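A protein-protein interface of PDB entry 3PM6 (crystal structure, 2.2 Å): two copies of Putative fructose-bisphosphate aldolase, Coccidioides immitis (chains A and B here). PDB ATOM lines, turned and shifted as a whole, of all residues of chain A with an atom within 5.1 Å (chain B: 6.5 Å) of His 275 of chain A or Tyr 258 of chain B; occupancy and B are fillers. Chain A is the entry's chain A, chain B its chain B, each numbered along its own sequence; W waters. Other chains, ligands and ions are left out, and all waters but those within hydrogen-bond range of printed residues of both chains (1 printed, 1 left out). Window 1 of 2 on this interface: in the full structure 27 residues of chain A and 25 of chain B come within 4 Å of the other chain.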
ATOM      1  N   GLU A  38     -17.193  -8.102   8.094  1.00  0.00           N
ATOM      2  CA  GLU A  38     -16.098  -8.703   7.357  1.00  0.00           C
ATOM      3  C   GLU A  38     -14.737  -8.204   7.876  1.00  0.00           C
ATOM      4  O   GLU A  38     -13.788  -8.971   7.989  1.00  0.00           O
ATOM      5  CB  GLU A  38     -16.216  -8.452   5.846  1.00  0.00           C
ATOM      6  CG  GLU A  38     -17.436  -9.085   5.201  1.00  0.00           C
ATOM      7  CD  GLU A  38     -18.614  -8.120   5.051  1.00  0.00           C
ATOM      8  OE1 GLU A  38     -18.851  -7.303   5.968  1.00  0.00           O
ATOM      9  OE2 GLU A  38     -19.314  -8.197   4.022  1.00  0.00           O
ATOM     10  N   TYR A 258     -11.563  -4.777   0.303  1.00  0.00           N
ATOM     11  CA  TYR A 258     -13.001  -5.034   0.257  1.00  0.00           C
ATOM     12  C   TYR A 258     -13.579  -4.438  -1.010  1.00  0.00           C
ATOM     13  O   TYR A 258     -14.364  -5.088  -1.700  1.00  0.00           O
ATOM     14  CB  TYR A 258     -13.675  -4.431   1.478  1.00  0.00           C
ATOM     15  CG  TYR A 258     -15.185  -4.399   1.504  1.00  0.00           C
ATOM     16  CD1 TYR A 258     -15.906  -3.396   0.839  1.00  0.00           C
ATOM     17  CD2 TYR A 258     -15.897  -5.331   2.262  1.00  0.00           C
ATOM     18  CE1 TYR A 258     -17.319  -3.352   0.900  1.00  0.00           C
ATOM     19  CE2 TYR A 258     -17.297  -5.294   2.348  1.00  0.00           C
ATOM     20  CZ  TYR A 258     -18.003  -4.307   1.664  1.00  0.00           C
ATOM     21  OH  TYR A 258     -19.379  -4.312   1.757  1.00  0.00           O
ATOM     22  N   MET A 262     -15.308  -6.477  -4.184  1.00  0.00           N
ATOM     23  CA  MET A 262     -16.696  -6.130  -4.537  1.00  0.00           C
ATOM     24  C   MET A 262     -16.774  -5.567  -5.959  1.00  0.00           C
ATOM     25  O   MET A 262     -17.661  -5.938  -6.727  1.00  0.00           O
ATOM     26  CB  MET A 262     -17.294  -5.117  -3.544  1.00  0.00           C
ATOM     27  CG  MET A 262     -17.620  -5.675  -2.163  1.00  0.00           C
ATOM     28  SD  MET A 262     -18.937  -6.901  -2.222  1.00  0.00           S
ATOM     29  CE  MET A 262     -19.051  -7.439  -0.522  1.00  0.00           C
ATOM     30  N   ILE A 271     -23.484 -14.489  -2.772  1.00  0.00           N
ATOM     31  CA  ILE A 271     -23.193 -13.563  -1.681  1.00  0.00           C
ATOM     32  C   ILE A 271     -22.290 -14.198  -0.626  1.00  0.00           C
ATOM     33  O   ILE A 271     -21.363 -13.543  -0.120  1.00  0.00           O
ATOM     34  CB  ILE A 271     -24.460 -13.018  -0.993  1.00  0.00           C
ATOM     35  CG1 ILE A 271     -25.216 -12.084  -1.920  1.00  0.00           C
ATOM     36  CG2 ILE A 271     -24.073 -12.192   0.264  1.00  0.00           C
ATOM     37  CD1 ILE A 271     -26.555 -11.606  -1.353  1.00  0.00           C
ATOM     38  N   THR A 272     -22.546 -15.463  -0.291  1.00  0.00           N
ATOM     39  CA  THR A 272     -21.716 -16.136   0.703  1.00  0.00           C
ATOM     40  C   THR A 272     -20.230 -16.097   0.337  1.00  0.00           C
ATOM     41  O   THR A 272     -19.391 -15.811   1.195  1.00  0.00           O
ATOM     42  CB  THR A 272     -22.139 -17.586   0.960  1.00  0.00           C
ATOM     43  OG1 THR A 272     -22.282 -18.272  -0.284  1.00  0.00           O
ATOM     44  CG2 THR A 272     -23.471 -17.667   1.756  1.00  0.00           C
ATOM     45  N   ARG A 273     -19.906 -16.393  -0.926  1.00  0.00           N
ATOM     46  CA  ARG A 273     -18.510 -16.390  -1.391  1.00  0.00           C
ATOM     47  C   ARG A 273     -17.963 -14.970  -1.484  1.00  0.00           C
ATOM     48  O   ARG A 273     -16.775 -14.726  -1.270  1.00  0.00           O
ATOM     49  CB  ARG A 273     -18.383 -17.095  -2.752  1.00  0.00           C
ATOM     50  CG  ARG A 273     -16.944 -17.352  -3.175  1.00  0.00           C
ATOM     51  CD  ARG A 273     -16.421 -18.653  -2.595  1.00  0.00           C
ATOM     52  NE  ARG A 273     -14.964 -18.735  -2.634  1.00  0.00           N
ATOM     53  CZ  ARG A 273     -14.181 -18.797  -1.558  1.00  0.00           C
ATOM     54  NH1 ARG A 273     -14.706 -18.790  -0.344  1.00  0.00           N
ATOM     55  NH2 ARG A 273     -12.860 -18.889  -1.696  1.00  0.00           N
ATOM     56  N   LEU A 274     -18.840 -14.034  -1.829  1.00  0.00           N
ATOM     57  CA  LEU A 274     -18.494 -12.615  -1.795  1.00  0.00           C
ATOM     58  C   LEU A 274     -17.971 -12.227  -0.407  1.00  0.00           C
ATOM     59  O   LEU A 274     -16.902 -11.632  -0.291  1.00  0.00           O
ATOM     60  CB  LEU A 274     -19.716 -11.799  -2.157  1.00  0.00           C
ATOM     61  CG  LEU A 274     -19.558 -10.581  -3.038  1.00  0.00           C
ATOM     62  CD1 LEU A 274     -18.724 -10.905  -4.268  1.00  0.00           C
ATOM     63  CD2 LEU A 274     -20.951 -10.092  -3.435  1.00  0.00           C
ATOM     64  N   HIS A 275     -18.693 -12.626   0.647  1.00  0.00           N
ATOM     65  CA  HIS A 275     -18.318 -12.270   2.017  1.00  0.00           C
ATOM     66  C   HIS A 275     -17.011 -12.931   2.397  1.00  0.00           C
ATOM     67  O   HIS A 275     -16.193 -12.328   3.077  1.00  0.00           O
ATOM     68  CB  HIS A 275     -19.407 -12.660   3.017  1.00  0.00           C
ATOM     69  CG  HIS A 275     -20.599 -11.760   2.976  1.00  0.00           C
ATOM     70  ND1 HIS A 275     -20.506 -10.399   3.154  1.00  0.00           N
ATOM     71  CD2 HIS A 275     -21.910 -12.023   2.787  1.00  0.00           C
ATOM     72  CE1 HIS A 275     -21.710  -9.857   3.061  1.00  0.00           C
ATOM     73  NE2 HIS A 275     -22.577 -10.820   2.823  1.00  0.00           N
ATOM     74  N   GLU A 276     -16.841 -14.178   1.960  1.00  0.00           N
ATOM     75  CA  GLU A 276     -15.627 -14.934   2.215  1.00  0.00           C
ATOM     76  C   GLU A 276     -14.418 -14.283   1.579  1.00  0.00           C
ATOM     77  O   GLU A 276     -13.370 -14.143   2.230  1.00  0.00           O
ATOM     78  CB  GLU A 276     -15.779 -16.391   1.748  1.00  0.00           C
ATOM     79  CG  GLU A 276     -16.723 -17.238   2.653  1.00  0.00           C
ATOM     80  CD  GLU A 276     -17.107 -18.615   2.051  1.00  0.00           C
ATOM     81  OE1 GLU A 276     -16.491 -19.069   1.045  1.00  0.00           O
ATOM     82  OE2 GLU A 276     -18.034 -19.240   2.595  1.00  0.00           O
ATOM     83  N   GLU A 277     -14.570 -13.870   0.322  1.00  0.00           N
ATOM     84  CA  GLU A 277     -13.446 -13.308  -0.435  1.00  0.00           C
ATOM     85  C   GLU A 277     -12.971 -11.934   0.091  1.00  0.00           C
ATOM     86  O   GLU A 277     -11.756 -11.724   0.249  1.00  0.00           O
ATOM     87  CB  GLU A 277     -13.729 -13.317  -1.957  1.00  0.00           C
ATOM     88  CG  GLU A 277     -13.772 -14.755  -2.534  1.00  0.00           C
ATOM     89  CD  GLU A 277     -13.658 -14.817  -4.065  1.00  0.00           C
ATOM     90  OE1 GLU A 277     -13.212 -13.824  -4.672  1.00  0.00           O
ATOM     91  OE2 GLU A 277     -14.019 -15.853  -4.663  1.00  0.00           O
ATOM     92  N   VAL A 278     -13.911 -11.037   0.432  1.00  0.00           N
ATOM     93  CA  VAL A 278     -13.522  -9.760   1.021  1.00  0.00           C
ATOM     94  C   VAL A 278     -12.821  -9.941   2.365  1.00  0.00           C
ATOM     95  O   VAL A 278     -11.874  -9.223   2.673  1.00  0.00           O
ATOM     96  CB  VAL A 278     -14.683  -8.721   1.127  1.00  0.00           C
ATOM     97  CG1 VAL A 278     -15.151  -8.309  -0.277  1.00  0.00           C
ATOM     98  CG2 VAL A 278     -15.857  -9.236   1.968  1.00  0.00           C
ATOM     99  N   THR A 279     -13.256 -10.922   3.149  1.00  0.00           N
ATOM    100  CA  THR A 279     -12.658 -11.149   4.450  1.00  0.00           C
ATOM    101  C   THR A 279     -11.232 -11.707   4.305  1.00  0.00           C
ATOM    102  O   THR A 279     -10.313 -11.237   4.988  1.00  0.00           O
ATOM    103  CB  THR A 279     -13.527 -12.098   5.278  1.00  0.00           C
ATOM    104  OG1 THR A 279     -14.873 -11.618   5.254  1.00  0.00           O
ATOM    105  CG2 THR A 279     -13.036 -12.166   6.703  1.00  0.00           C
ATOM    106  N   TYR B  35     -27.521 -12.596   5.230  1.00  0.00           N
ATOM    107  CA  TYR B  35     -26.140 -13.085   5.242  1.00  0.00           C
ATOM    108  C   TYR B  35     -25.193 -12.138   5.970  1.00  0.00           C
ATOM    109  O   TYR B  35     -23.985 -12.403   6.118  1.00  0.00           O
ATOM    110  CB  TYR B  35     -25.635 -13.310   3.805  1.00  0.00           C
ATOM    111  CG  TYR B  35     -26.432 -14.339   3.043  1.00  0.00           C
ATOM    112  CD1 TYR B  35     -26.125 -15.689   3.151  1.00  0.00           C
ATOM    113  CD2 TYR B  35     -27.517 -13.953   2.213  1.00  0.00           C
ATOM    114  CE1 TYR B  35     -26.862 -16.662   2.458  1.00  0.00           C
ATOM    115  CE2 TYR B  35     -28.261 -14.912   1.513  1.00  0.00           C
ATOM    116  CZ  TYR B  35     -27.920 -16.270   1.639  1.00  0.00           C
ATOM    117  OH  TYR B  35     -28.638 -17.242   0.969  1.00  0.00           O
ATOM    118  N   ASN B  36     -25.743 -11.033   6.450  1.00  0.00           N
ATOM    119  CA  ASN B  36     -24.899  -9.949   6.931  1.00  0.00           C
ATOM    120  C   ASN B  36     -25.623  -9.019   7.893  1.00  0.00           C
ATOM    121  O   ASN B  36     -26.852  -9.040   7.980  1.00  0.00           O
ATOM    122  CB  ASN B  36     -24.382  -9.161   5.730  1.00  0.00           C
ATOM    123  CG  ASN B  36     -25.458  -8.938   4.654  1.00  0.00           C
ATOM    124  OD1 ASN B  36     -26.537  -8.403   4.930  1.00  0.00           O
ATOM    125  ND2 ASN B  36     -25.152  -9.354   3.405  1.00  0.00           N
ATOM    126  N   GLU B  38     -26.036  -5.774   7.465  1.00  0.00           N
ATOM    127  CA  GLU B  38     -26.920  -4.906   6.654  1.00  0.00           C
ATOM    128  C   GLU B  38     -28.313  -5.511   6.510  1.00  0.00           C
ATOM    129  O   GLU B  38     -29.295  -4.794   6.564  1.00  0.00           O
ATOM    130  CB  GLU B  38     -26.332  -4.622   5.261  1.00  0.00           C
ATOM    131  CG  GLU B  38     -24.975  -3.902   5.236  1.00  0.00           C
ATOM    132  CD  GLU B  38     -23.798  -4.842   4.961  1.00  0.00           C
ATOM    133  OE1 GLU B  38     -23.745  -5.933   5.559  1.00  0.00           O
ATOM    134  OE2 GLU B  38     -22.910  -4.486   4.162  1.00  0.00           O
ATOM    135  N   GLY B  39     -28.396  -6.834   6.355  1.00  0.00           N
ATOM    136  CA  GLY B  39     -29.680  -7.520   6.234  1.00  0.00           C
ATOM    137  C   GLY B  39     -30.453  -7.441   7.549  1.00  0.00           C
ATOM    138  O   GLY B  39     -31.635  -7.143   7.546  1.00  0.00           O
ATOM    139  N   TRP B  61     -24.238 -21.714   7.055  1.00  0.00           N
ATOM    140  CA  TRP B  61     -23.088 -20.929   6.648  1.00  0.00           C
ATOM    141  C   TRP B  61     -22.778 -19.751   7.599  1.00  0.00           C
ATOM    142  O   TRP B  61     -21.619 -19.437   7.800  1.00  0.00           O
ATOM    143  CB  TRP B  61     -23.250 -20.420   5.228  1.00  0.00           C
ATOM    144  CG  TRP B  61     -22.196 -19.371   4.830  1.00  0.00           C
ATOM    145  CD1 TRP B  61     -21.002 -19.605   4.198  1.00  0.00           C
ATOM    146  CD2 TRP B  61     -22.291 -17.935   4.997  1.00  0.00           C
ATOM    147  NE1 TRP B  61     -20.339 -18.403   3.978  1.00  0.00           N
ATOM    148  CE2 TRP B  61     -21.100 -17.370   4.469  1.00  0.00           C
ATOM    149  CE3 TRP B  61     -23.260 -17.077   5.568  1.00  0.00           C
ATOM    150  CZ2 TRP B  61     -20.843 -15.980   4.495  1.00  0.00           C
ATOM    151  CZ3 TRP B  61     -23.014 -15.680   5.593  1.00  0.00           C
ATOM    152  CH2 TRP B  61     -21.806 -15.148   5.056  1.00  0.00           C
ATOM    153  N   TYR B  65     -19.106 -19.473   8.927  1.00  0.00           N
ATOM    154  CA  TYR B  65     -18.338 -18.294   8.571  1.00  0.00           C
ATOM    155  C   TYR B  65     -17.938 -17.459   9.797  1.00  0.00           C
ATOM    156  O   TYR B  65     -16.775 -17.119   9.956  1.00  0.00           O
ATOM    157  CB  TYR B  65     -19.154 -17.479   7.559  1.00  0.00           C
ATOM    158  CG  TYR B  65     -18.682 -16.067   7.314  1.00  0.00           C
ATOM    159  CD1 TYR B  65     -17.512 -15.829   6.600  1.00  0.00           C
ATOM    160  CD2 TYR B  65     -19.416 -14.969   7.769  1.00  0.00           C
ATOM    161  CE1 TYR B  65     -17.077 -14.547   6.347  1.00  0.00           C
ATOM    162  CE2 TYR B  65     -18.990 -13.663   7.496  1.00  0.00           C
ATOM    163  CZ  TYR B  65     -17.805 -13.473   6.784  1.00  0.00           C
ATOM    164  OH  TYR B  65     -17.299 -12.220   6.516  1.00  0.00           O
ATOM    165  N   VAL B 254     -35.061 -10.076  -1.369  1.00  0.00           N
ATOM    166  CA  VAL B 254     -34.424  -9.097  -0.506  1.00  0.00           C
ATOM    167  C   VAL B 254     -32.917  -8.952  -0.798  1.00  0.00           C
ATOM    168  O   VAL B 254     -32.430  -7.854  -1.037  1.00  0.00           O
ATOM    169  CB  VAL B 254     -34.644  -9.439   0.994  1.00  0.00           C
ATOM    170  CG1 VAL B 254     -33.857  -8.466   1.898  1.00  0.00           C
ATOM    171  CG2 VAL B 254     -36.151  -9.460   1.337  1.00  0.00           C
ATOM    172  N   ASN B 255     -32.187 -10.058  -0.769  1.00  0.00           N
ATOM    173  CA  ASN B 255     -30.737 -10.022  -0.939  1.00  0.00           C
ATOM    174  C   ASN B 255     -30.219  -9.622  -2.309  1.00  0.00           C
ATOM    175  O   ASN B 255     -29.096  -9.116  -2.425  1.00  0.00           O
ATOM    176  CB  ASN B 255     -30.116 -11.339  -0.488  1.00  0.00           C
ATOM    177  CG  ASN B 255     -30.219 -11.508   1.004  1.00  0.00           C
ATOM    178  OD1 ASN B 255     -29.688 -10.684   1.767  1.00  0.00           O
ATOM    179  ND2 ASN B 255     -30.948 -12.523   1.436  1.00  0.00           N
ATOM    180  N   ASN B 256     -31.027  -9.834  -3.342  1.00  0.00           N
ATOM    181  CA  ASN B 256     -30.638  -9.344  -4.664  1.00  0.00           C
ATOM    182  C   ASN B 256     -30.495  -7.826  -4.703  1.00  0.00           C
ATOM    183  O   ASN B 256     -29.747  -7.315  -5.521  1.00  0.00           O
ATOM    184  CB  ASN B 256     -31.603  -9.815  -5.760  1.00  0.00           C
ATOM    185  CG  ASN B 256     -30.981 -10.848  -6.640  1.00  0.00           C
ATOM    186  OD1 ASN B 256     -31.178 -12.060  -6.429  1.00  0.00           O
ATOM    187  ND2 ASN B 256     -30.173 -10.387  -7.630  1.00  0.00           N
ATOM    188  N   GLU B 257     -31.182  -7.122  -3.799  1.00  0.00           N
ATOM    189  CA  GLU B 257     -31.031  -5.659  -3.704  1.00  0.00           C
ATOM    190  C   GLU B 257     -29.628  -5.289  -3.237  1.00  0.00           C
ATOM    191  O   GLU B 257     -29.080  -4.265  -3.634  1.00  0.00           O
ATOM    192  CB  GLU B 257     -32.069  -5.033  -2.761  1.00  0.00           C
ATOM    193  CG  GLU B 257     -33.481  -5.174  -3.216  1.00  0.00           C
ATOM    194  CD  GLU B 257     -33.706  -4.598  -4.610  1.00  0.00           C
ATOM    195  OE1 GLU B 257     -33.499  -3.385  -4.819  1.00  0.00           O
ATOM    196  OE2 GLU B 257     -34.080  -5.370  -5.503  1.00  0.00           O
ATOM    197  N   TYR B 258     -29.060  -6.130  -2.371  1.00  0.00           N
ATOM    198  CA  TYR B 258     -27.732  -5.910  -1.859  1.00  0.00           C
ATOM    199  C   TYR B 258     -26.772  -6.100  -3.019  1.00  0.00           C
ATOM    200  O   TYR B 258     -25.830  -5.320  -3.171  1.00  0.00           O
ATOM    201  CB  TYR B 258     -27.412  -6.871  -0.694  1.00  0.00           C
ATOM    202  CG  TYR B 258     -25.942  -6.957  -0.294  1.00  0.00           C
ATOM    203  CD1 TYR B 258     -25.025  -7.691  -1.049  1.00  0.00           C
ATOM    204  CD2 TYR B 258     -25.483  -6.348   0.864  1.00  0.00           C
ATOM    205  CE1 TYR B 258     -23.679  -7.787  -0.673  1.00  0.00           C
ATOM    206  CE2 TYR B 258     -24.134  -6.445   1.251  1.00  0.00           C
ATOM    207  CZ  TYR B 258     -23.253  -7.166   0.482  1.00  0.00           C
ATOM    208  OH  TYR B 258     -21.932  -7.240   0.875  1.00  0.00           O
ATOM    209  N   VAL B 259     -27.003  -7.138  -3.815  1.00  0.00           N
ATOM    210  CA  VAL B 259     -26.111  -7.463  -4.940  1.00  0.00           C
ATOM    211  C   VAL B 259     -26.188  -6.389  -6.026  1.00  0.00           C
ATOM    212  O   VAL B 259     -25.168  -6.019  -6.596  1.00  0.00           O
ATOM    213  CB  VAL B 259     -26.414  -8.872  -5.518  1.00  0.00           C
ATOM    214  CG1 VAL B 259     -25.616  -9.133  -6.771  1.00  0.00           C
ATOM    215  CG2 VAL B 259     -26.102  -9.954  -4.492  1.00  0.00           C
ATOM    216  N   LYS B 260     -27.389  -5.870  -6.283  1.00  0.00           N
ATOM    217  CA  LYS B 260     -27.563  -4.854  -7.318  1.00  0.00           C
ATOM    218  C   LYS B 260     -26.746  -3.622  -6.987  1.00  0.00           C
ATOM    219  O   LYS B 260     -25.949  -3.182  -7.819  1.00  0.00           O
ATOM    220  CB  LYS B 260     -29.045  -4.501  -7.563  1.00  0.00           C
ATOM    221  N   VAL B 261     -26.920  -3.071  -5.779  1.00  0.00           N
ATOM    222  CA  VAL B 261     -26.156  -1.877  -5.383  1.00  0.00           C
ATOM    223  C   VAL B 261     -24.631  -2.080  -5.554  1.00  0.00           C
ATOM    224  O   VAL B 261     -23.982  -1.242  -6.140  1.00  0.00           O
ATOM    225  CB  VAL B 261     -26.519  -1.401  -3.950  1.00  0.00           C
ATOM    226  CG1 VAL B 261     -25.595  -0.296  -3.467  1.00  0.00           C
ATOM    227  CG2 VAL B 261     -27.958  -0.900  -3.906  1.00  0.00           C
ATOM    228  N   MET B 262     -24.077  -3.188  -5.056  1.00  0.00           N
ATOM    229  CA  MET B 262     -22.620  -3.474  -5.139  1.00  0.00           C
ATOM    230  C   MET B 262     -22.127  -3.657  -6.574  1.00  0.00           C
ATOM    231  O   MET B 262     -21.045  -3.203  -6.906  1.00  0.00           O
ATOM    232  CB  MET B 262     -22.254  -4.746  -4.356  1.00  0.00           C
ATOM    233  CG  MET B 262     -22.459  -4.694  -2.839  1.00  0.00           C
ATOM    234  SD  MET B 262     -21.441  -3.415  -2.080  1.00  0.00           S
ATOM    235  CE  MET B 262     -21.665  -3.785  -0.350  1.00  0.00           C
ATOM    236  N   ARG B 263     -22.911  -4.348  -7.411  1.00  0.00           N
ATOM    237  CA  ARG B 263     -22.611  -4.486  -8.832  1.00  0.00           C
ATOM    238  C   ARG B 263     -22.532  -3.092  -9.460  1.00  0.00           C
ATOM    239  O   ARG B 263     -21.556  -2.752 -10.124  1.00  0.00           O
ATOM    240  CB  ARG B 263     -23.673  -5.371  -9.541  1.00  0.00           C
ATOM    241  CG  ARG B 263     -23.099  -6.271 -10.668  1.00  0.00           C
ATOM    242  CD  ARG B 263     -24.129  -6.670 -11.747  1.00  0.00           C
ATOM    243  NE  ARG B 263     -24.972  -7.810 -11.369  1.00  0.00           N
ATOM    244  CZ  ARG B 263     -26.254  -7.738 -10.983  1.00  0.00           C
ATOM    245  NH1 ARG B 263     -26.889  -6.560 -10.930  1.00  0.00           N
ATOM    246  NH2 ARG B 263     -26.912  -8.854 -10.663  1.00  0.00           N
ATOM    247  N   HIS B 275     -22.775   0.728   2.466  1.00  0.00           N
ATOM    248  CA  HIS B 275     -23.527   0.066   3.560  1.00  0.00           C
ATOM    249  C   HIS B 275     -24.930   0.669   3.700  1.00  0.00           C
ATOM    250  O   HIS B 275     -25.905  -0.066   3.801  1.00  0.00           O
ATOM    251  CB  HIS B 275     -22.758   0.023   4.909  1.00  0.00           C
ATOM    252  CG  HIS B 275     -21.545  -0.858   4.877  1.00  0.00           C
ATOM    253  ND1 HIS B 275     -21.583  -2.169   4.435  1.00  0.00           N
ATOM    254  CD2 HIS B 275     -20.253  -0.615   5.207  1.00  0.00           C
ATOM    255  CE1 HIS B 275     -20.370  -2.687   4.488  1.00  0.00           C
ATOM    256  NE2 HIS B 275     -19.548  -1.769   4.955  1.00  0.00           N
ATOM    257  N   VAL B 278     -27.060  -0.366   0.417  1.00  0.00           N
ATOM    258  CA  VAL B 278     -27.543  -1.756   0.442  1.00  0.00           C
ATOM    259  C   VAL B 278     -28.624  -1.985   1.519  1.00  0.00           C
ATOM    260  O   VAL B 278     -29.615  -2.658   1.267  1.00  0.00           O
ATOM    261  CB  VAL B 278     -26.392  -2.830   0.514  1.00  0.00           C
ATOM    262  CG1 VAL B 278     -25.415  -2.599  -0.621  1.00  0.00           C
ATOM    263  CG2 VAL B 278     -25.668  -2.808   1.873  1.00  0.00           C
ATOM    264  N   THR B 279     -28.438  -1.420   2.704  1.00  0.00           N
ATOM    265  CA  THR B 279     -29.437  -1.529   3.786  1.00  0.00           C
ATOM    266  C   THR B 279     -30.799  -0.920   3.399  1.00  0.00           C
ATOM    267  O   THR B 279     -31.804  -1.559   3.586  1.00  0.00           O
ATOM    268  CB  THR B 279     -28.930  -0.876   5.090  1.00  0.00           C
ATOM    269  OG1 THR B 279     -27.599  -1.323   5.343  1.00  0.00           O
ATOM    270  CG2 THR B 279     -29.787  -1.275   6.278  1.00  0.00           C
ATOM    271  N   ALA B 281     -31.970  -0.290   0.282  1.00  0.00           N
ATOM    272  CA  ALA B 281     -32.501  -1.138  -0.771  1.00  0.00           C
ATOM    273  C   ALA B 281     -33.116  -2.421  -0.207  1.00  0.00           C
ATOM    274  O   ALA B 281     -34.246  -2.814  -0.596  1.00  0.00           O
ATOM    275  CB  ALA B 281     -31.432  -1.448  -1.850  1.00  0.00           C
ATOM    276  N   MET B 282     -32.395  -3.081   0.700  1.00  0.00           N
ATOM    277  CA  MET B 282     -32.953  -4.273   1.308  1.00  0.00           C
ATOM    278  C   MET B 282     -34.178  -3.970   2.164  1.00  0.00           C
ATOM    279  O   MET B 282     -35.155  -4.741   2.149  1.00  0.00           O
ATOM    280  CB  MET B 282     -31.920  -5.034   2.098  1.00  0.00           C
ATOM    281  CG  MET B 282     -30.945  -5.759   1.217  1.00  0.00           C
ATOM    282  SD  MET B 282     -29.897  -6.892   2.128  1.00  0.00           S
ATOM    283  CE  MET B 282     -28.881  -5.773   3.079  1.00  0.00           C
HETATM  284  O   HOH W   1     -20.870  -6.090   3.038  1.00  0.00           O
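The backbone carbonyl oxygen of His 275 of chain A is in hydrogen-bond range of the side-chain hydroxyl of Thr 279 of chain A, at 2.6 Å. OE2 of Glu 38 of chain B sits at hydrogen-bond distance from ND1 of His 275 of chain B (2.7 Å). The side-chain hydroxyl (OG1) of Thr 279 of chain B is in hydrogen-bond range of the backbone carbonyl oxygen (O) of His 275 of chain B (2.6 Å). The guanidinium group (NE) of Arg 273 of chain A is in salt-bridge range of the side-chain carboxylate (OE1) of Glu 276 of chain A, 3.997 Å away. The side-chain amide oxygen (OD1) of Asn 36 of chain B lies within hydrogen-bond range of the backbone NH (N) of Gly 39 of chain B (2.8 Å). The side-chain carboxylate of Glu 38 of chain A lies within hydrogen-bond range of a ring nitrogen (ND1) of His 275 of chain A, at 2.7 Å.
Printed residues of chain B that touch a printed residue of chain A: Tyr 35, Asn 36, Trp 61, Tyr 65, Asn 255, Tyr 258, Val 259, Met 262 and His 275. Among the printed residues, 16 pairs touch across the chains. Among the printed residues, no Asp or Glu carboxylate lies within 4 Å of a Lys or Arg side-chain nitrogen of the other chain.
Glu 38 of chain A touches Tyr 65 of chain B. Tyr 258 of chain A touches Tyr 258 of chain B (OH to OH, 3.98 Å). Tyr 258 of chain A touches His 275 of chain B. Met 262 of chain A touches Tyr 258 of chain B. Ile 271 of chain A touches Val 259 of chain B. Thr 272 of chain A touches Tyr 35 of chain B (CG2 to CD1, 3.6 Å). Trp 61 of chain B touches Thr 272 of chain A. His 275 of chain A touches Tyr 35 of chain B (NE2 to O, 3.9 Å). His 275 of chain A touches Trp 61 of chain B. Tyr 258 of chain B touches His 275 of chain A.
Tyr 258 of chain B touches its own counterpart, Tyr 258 of chain A. Tyr 258 of chain A touches Met 262 of chain B, and with the chains exchanged Met 262 of chain A touches Tyr 258 of chain B. Tyr 258 of chain A touches His 275 of chain B, and with the chains exchanged His 275 of chain A touches Tyr 258 of chain B. Positions printed for both chains: 38, 258, 262, 275, 278 and 279. Of the 16 pairs that touch across the chains among the printed residues, 5 have their exchanged pair printed and touching as well.
Of the printed residues of chain A, Tyr 258 of chain B touches Tyr 258, Met 262 and His 275. Printed residues of chain A within 4 Å of Tyr 65 of chain B: Glu 38 (3.4 Å), His 275 (3.6 Å) and Thr 279 (2.8 Å). Of the printed residues of chain B, Glu 38 of chain A touches Tyr 65. Of the printed residues of chain B, Thr 272 of chain A touches Tyr 35 (3.6 Å) and Trp 61 (3.5 Å). Glu 38 of chain B touches none of the printed residues of chain A. The nearest residue of chain B that does not touch His 275 of chain A is Glu 38 of chain B (5.1 Å). The nearest printed residue of chain B that does not touch Glu 38 of chain A is Tyr 258 of chain B (4.2 Å).
The side-chain hydroxyl of Thr 279 of chain A sits at hydrogen-bond distance from the side-chain hydroxyl of Tyr 65 of chain B (2.8 Å). NE1 of Trp 61 of chain B sits at hydrogen-bond distance from OE2 of Glu 276 of chain A, at 2.8 Å. NE2 of His 275 of chain A is in hydrogen-bond range of ND2 of Asn 36 of chain B, 3.0 Å away.
Water W1 lies within hydrogen-bond range of the side-chain hydroxyl (OH) of Tyr 258 of chain A, the side-chain hydroxyl (OH) of Tyr 258 of chain B, the side-chain carboxylate (OE2) of Glu 38 of chain A and the side-chain carboxylate (OE2) of Glu 38 of chain B.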
